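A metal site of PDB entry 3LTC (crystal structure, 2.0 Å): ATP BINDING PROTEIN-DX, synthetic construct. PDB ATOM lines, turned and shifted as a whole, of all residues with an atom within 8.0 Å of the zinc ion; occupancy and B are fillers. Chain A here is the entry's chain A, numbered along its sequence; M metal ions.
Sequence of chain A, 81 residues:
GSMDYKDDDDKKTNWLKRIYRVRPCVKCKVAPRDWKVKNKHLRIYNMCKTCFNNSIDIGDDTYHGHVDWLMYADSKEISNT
The backbone NH (N) of Cys 25 lies within hydrogen-bond range of the backbone carbonyl oxygen (O) of Ala 31 (2.8 Å). SG of Cys 48 lies close to N of Thr 50 (3.7 Å). The side-chain sulfur of Cys 25 lies close to the backbone NH of Lys 27 (3.3 Å). The side-chain sulfur of Cys 28 lies close to the backbone NH of Val 30 (3.6 Å). N of Ala 31 lies close to SG of Cys 28.
Four residues have an atom within 4 Å of the zinc ion: Cys 25, Cys 28, Cys 48 and Cys 51.
The zinc ion is bound by SG of Cys 51 (2.3 Å), SG of Cys 48 (2.4 Å), SG of Cys 25 (2.4 Å) and SG of Cys 28 (2.4 Å).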
ATOM      1  N   PRO A  24     -13.858   7.258  21.307  1.00  0.00           N
ATOM      2  CA  PRO A  24     -13.435   7.242  19.897  1.00  0.00           C
ATOM      3  C   PRO A  24     -12.311   6.215  19.611  1.00  0.00           C
ATOM      4  O   PRO A  24     -11.845   5.501  20.509  1.00  0.00           O
ATOM      5  CB  PRO A  24     -12.922   8.688  19.683  1.00  0.00           C
ATOM      6  CG  PRO A  24     -12.427   9.102  21.070  1.00  0.00           C
ATOM      7  CD  PRO A  24     -13.399   8.458  22.037  1.00  0.00           C
ATOM      8  N   CYS A  25     -11.889   6.176  18.345  1.00  0.00           N
ATOM      9  CA  CYS A  25     -10.807   5.316  17.909  1.00  0.00           C
ATOM     10  C   CYS A  25      -9.676   5.317  18.935  1.00  0.00           C
ATOM     11  O   CYS A  25      -9.267   6.394  19.401  1.00  0.00           O
ATOM     12  CB  CYS A  25     -10.310   5.864  16.564  1.00  0.00           C
ATOM     13  SG  CYS A  25      -8.890   5.005  15.955  1.00  0.00           S
ATOM     14  N   VAL A  26      -9.182   4.125  19.291  1.00  0.00           N
ATOM     15  CA  VAL A  26      -8.085   4.019  20.280  1.00  0.00           C
ATOM     16  C   VAL A  26      -6.743   4.528  19.733  1.00  0.00           C
ATOM     17  O   VAL A  26      -5.795   4.727  20.511  1.00  0.00           O
ATOM     18  CB  VAL A  26      -7.853   2.561  20.734  1.00  0.00           C
ATOM     19  CG1 VAL A  26      -9.124   2.001  21.444  1.00  0.00           C
ATOM     20  CG2 VAL A  26      -7.410   1.688  19.560  1.00  0.00           C
ATOM     21  N   LYS A  27      -6.659   4.723  18.428  1.00  0.00           N
ATOM     22  CA  LYS A  27      -5.395   5.162  17.801  1.00  0.00           C
ATOM     23  C   LYS A  27      -5.359   6.679  17.585  1.00  0.00           C
ATOM     24  O   LYS A  27      -4.468   7.382  18.072  1.00  0.00           O
ATOM     25  CB  LYS A  27      -5.147   4.426  16.463  1.00  0.00           C
ATOM     26  CG  LYS A  27      -3.764   4.791  15.814  1.00  0.00           C
ATOM     27  CD  LYS A  27      -2.604   4.206  16.584  1.00  0.00           C
ATOM     28  CE  LYS A  27      -1.241   4.776  16.021  1.00  0.00           C
ATOM     29  NZ  LYS A  27      -0.092   4.384  16.915  1.00  0.00           N
ATOM     30  N   CYS A  28      -6.305   7.212  16.832  1.00  0.00           N
ATOM     31  CA  CYS A  28      -6.270   8.652  16.565  1.00  0.00           C
ATOM     32  C   CYS A  28      -6.980   9.426  17.658  1.00  0.00           C
ATOM     33  O   CYS A  28      -6.785  10.642  17.784  1.00  0.00           O
ATOM     34  CB  CYS A  28      -6.863   9.020  15.192  1.00  0.00           C
ATOM     35  SG  CYS A  28      -8.665   8.724  15.065  1.00  0.00           S
ATOM     36  N   LYS A  29      -7.779   8.704  18.426  1.00  0.00           N
ATOM     37  CA  LYS A  29      -8.523   9.279  19.568  1.00  0.00           C
ATOM     38  C   LYS A  29      -9.486  10.395  19.180  1.00  0.00           C
ATOM     39  O   LYS A  29      -9.882  11.189  20.031  1.00  0.00           O
ATOM     40  CB  LYS A  29      -7.525   9.738  20.647  1.00  0.00           C
ATOM     41  CG  LYS A  29      -6.937   8.525  21.381  1.00  0.00           C
ATOM     42  CD  LYS A  29      -5.559   8.684  21.879  1.00  0.00           C
ATOM     43  CE  LYS A  29      -5.216   7.404  22.637  1.00  0.00           C
ATOM     44  NZ  LYS A  29      -4.049   7.594  23.528  1.00  0.00           N
ATOM     45  N   VAL A  30      -9.897  10.442  17.924  1.00  0.00           N
ATOM     46  CA  VAL A  30     -10.820  11.491  17.500  1.00  0.00           C
ATOM     47  C   VAL A  30     -11.998  10.909  16.694  1.00  0.00           C
ATOM     48  O   VAL A  30     -13.163  11.121  17.047  1.00  0.00           O
ATOM     49  CB  VAL A  30     -10.082  12.593  16.675  1.00  0.00           C
ATOM     50  CG1 VAL A  30     -11.051  13.388  15.821  1.00  0.00           C
ATOM     51  CG2 VAL A  30      -9.281  13.516  17.645  1.00  0.00           C
ATOM     52  N   ALA A  31     -11.707  10.165  15.630  1.00  0.00           N
ATOM     53  CA  ALA A  31     -12.784   9.593  14.808  1.00  0.00           C
ATOM     54  C   ALA A  31     -13.544   8.504  15.542  1.00  0.00           C
ATOM     55  O   ALA A  31     -12.972   7.780  16.373  1.00  0.00           O
ATOM     56  CB  ALA A  31     -12.209   9.010  13.483  1.00  0.00           C
ATOM     57  N   PRO A  32     -14.838   8.354  15.232  1.00  0.00           N
ATOM     58  CA  PRO A  32     -15.539   7.171  15.788  1.00  0.00           C
ATOM     59  C   PRO A  32     -15.046   5.833  15.236  1.00  0.00           C
ATOM     60  O   PRO A  32     -14.419   5.791  14.173  1.00  0.00           O
ATOM     61  CB  PRO A  32     -17.019   7.426  15.449  1.00  0.00           C
ATOM     62  CG  PRO A  32     -16.996   8.432  14.346  1.00  0.00           C
ATOM     63  CD  PRO A  32     -15.660   9.123  14.283  1.00  0.00           C
ATOM     64  N   ARG A  33     -15.358   4.741  15.938  1.00  0.00           N
ATOM     65  CA  ARG A  33     -14.860   3.403  15.588  1.00  0.00           C
ATOM     66  C   ARG A  33     -15.633   2.756  14.433  1.00  0.00           C
ATOM     67  O   ARG A  33     -16.825   3.010  14.249  1.00  0.00           O
ATOM     68  CB  ARG A  33     -14.922   2.488  16.815  1.00  0.00           C
ATOM     69  CG  ARG A  33     -13.939   2.966  17.892  1.00  0.00           C
ATOM     70  CD  ARG A  33     -14.077   2.170  19.193  1.00  0.00           C
ATOM     71  NE  ARG A  33     -13.309   2.877  20.239  1.00  0.00           N
ATOM     72  CZ  ARG A  33     -12.945   2.349  21.408  1.00  0.00           C
ATOM     73  NH1 ARG A  33     -13.244   1.105  21.694  1.00  0.00           N
ATOM     74  NH2 ARG A  33     -12.305   3.101  22.302  1.00  0.00           N
ATOM     75  N   ASP A  34     -14.944   1.899  13.673  1.00  0.00           N
ATOM     76  CA  ASP A  34     -15.658   1.082  12.735  1.00  0.00           C
ATOM     77  C   ASP A  34     -16.472   0.076  13.546  1.00  0.00           C
ATOM     78  O   ASP A  34     -16.222  -0.129  14.742  1.00  0.00           O
ATOM     79  CB  ASP A  34     -14.706   0.358  11.781  1.00  0.00           C
ATOM     80  CG  ASP A  34     -15.458  -0.254  10.566  1.00  0.00           C
ATOM     81  OD1 ASP A  34     -16.583   0.189  10.246  1.00  0.00           O
ATOM     82  OD2 ASP A  34     -14.905  -1.157   9.952  1.00  0.00           O
ATOM     83  N   ASN A  46     -11.893  -1.602  17.519  1.00  0.00           N
ATOM     84  CA  ASN A  46     -11.173  -0.671  18.366  1.00  0.00           C
ATOM     85  C   ASN A  46     -10.779   0.614  17.631  1.00  0.00           C
ATOM     86  O   ASN A  46     -10.640   1.635  18.276  1.00  0.00           O
ATOM     87  CB  ASN A  46      -9.940  -1.304  19.013  1.00  0.00           C
ATOM     88  CG  ASN A  46     -10.297  -2.430  19.966  1.00  0.00           C
ATOM     89  OD1 ASN A  46     -11.427  -2.506  20.429  1.00  0.00           O
ATOM     90  ND2 ASN A  46      -9.338  -3.319  20.270  1.00  0.00           N
ATOM     91  N   MET A  47     -10.639   0.552  16.311  1.00  0.00           N
ATOM     92  CA  MET A  47     -10.182   1.721  15.514  1.00  0.00           C
ATOM     93  C   MET A  47     -11.189   2.187  14.475  1.00  0.00           C
ATOM     94  O   MET A  47     -12.025   1.377  14.040  1.00  0.00           O
ATOM     95  CB  MET A  47      -8.866   1.383  14.778  1.00  0.00           C
ATOM     96  CG  MET A  47      -7.635   1.427  15.729  1.00  0.00           C
ATOM     97  SD  MET A  47      -6.055   1.151  14.863  1.00  0.00           S
ATOM     98  CE  MET A  47      -6.294  -0.590  14.513  1.00  0.00           C
ATOM     99  N   CYS A  48     -11.081   3.461  14.068  1.00  0.00           N
ATOM    100  CA  CYS A  48     -11.808   3.940  12.902  1.00  0.00           C
ATOM    101  C   CYS A  48     -11.207   3.182  11.680  1.00  0.00           C
ATOM    102  O   CYS A  48     -10.146   2.504  11.812  1.00  0.00           O
ATOM    103  CB  CYS A  48     -11.680   5.473  12.732  1.00  0.00           C
ATOM    104  SG  CYS A  48      -9.994   6.029  12.280  1.00  0.00           S
ATOM    105  N   LYS A  49     -11.852   3.279  10.517  1.00  0.00           N
ATOM    106  CA  LYS A  49     -11.347   2.550   9.342  1.00  0.00           C
ATOM    107  C   LYS A  49     -10.000   3.119   8.862  1.00  0.00           C
ATOM    108  O   LYS A  49      -9.125   2.365   8.454  1.00  0.00           O
ATOM    109  CB  LYS A  49     -12.352   2.599   8.168  1.00  0.00           C
ATOM    110  CG  LYS A  49     -12.013   1.588   7.059  1.00  0.00           C
ATOM    111  CD  LYS A  49     -12.510   0.173   7.528  1.00  0.00           C
ATOM    112  CE  LYS A  49     -11.996  -0.930   6.652  1.00  0.00           C
ATOM    113  NZ  LYS A  49     -12.503  -2.256   7.135  1.00  0.00           N
ATOM    114  N   THR A  50      -9.826   4.441   8.921  1.00  0.00           N
ATOM    115  CA  THR A  50      -8.590   5.076   8.457  1.00  0.00           C
ATOM    116  C   THR A  50      -7.409   4.542   9.247  1.00  0.00           C
ATOM    117  O   THR A  50      -6.376   4.154   8.658  1.00  0.00           O
ATOM    118  CB  THR A  50      -8.659   6.581   8.624  1.00  0.00           C
ATOM    119  OG1 THR A  50      -9.819   7.049   7.960  1.00  0.00           O
ATOM    120  CG2 THR A  50      -7.382   7.306   8.076  1.00  0.00           C
ATOM    121  N   CYS A  51      -7.519   4.536  10.586  1.00  0.00           N
ATOM    122  CA  CYS A  51      -6.399   4.025  11.401  1.00  0.00           C
ATOM    123  C   CYS A  51      -6.207   2.515  11.242  1.00  0.00           C
ATOM    124  O   CYS A  51      -5.079   2.022  11.296  1.00  0.00           O
ATOM    125  CB  CYS A  51      -6.574   4.372  12.884  1.00  0.00           C
ATOM    126  SG  CYS A  51      -6.432   6.169  13.217  1.00  0.00           S
ATOM    127  N   PHE A  52      -7.307   1.774  11.090  1.00  0.00           N
ATOM    128  CA  PHE A  52      -7.166   0.334  10.858  1.00  0.00           C
ATOM    129  C   PHE A  52      -6.427   0.029   9.525  1.00  0.00           C
ATOM    130  O   PHE A  52      -5.485  -0.774   9.481  1.00  0.00           O
ATOM    131  CB  PHE A  52      -8.525  -0.369  10.852  1.00  0.00           C
ATOM    132  CG  PHE A  52      -8.403  -1.800  10.451  1.00  0.00           C
ATOM    133  CD1 PHE A  52      -7.819  -2.727  11.303  1.00  0.00           C
ATOM    134  CD2 PHE A  52      -8.763  -2.191   9.169  1.00  0.00           C
ATOM    135  CE1 PHE A  52      -7.665  -4.085  10.902  1.00  0.00           C
ATOM    136  CE2 PHE A  52      -8.616  -3.541   8.760  1.00  0.00           C
ATOM    137  CZ  PHE A  52      -8.071  -4.486   9.618  1.00  0.00           C
HETATM  138 ZN    ZN M   1      -8.570   6.493  14.094  1.00  0.00          ZN
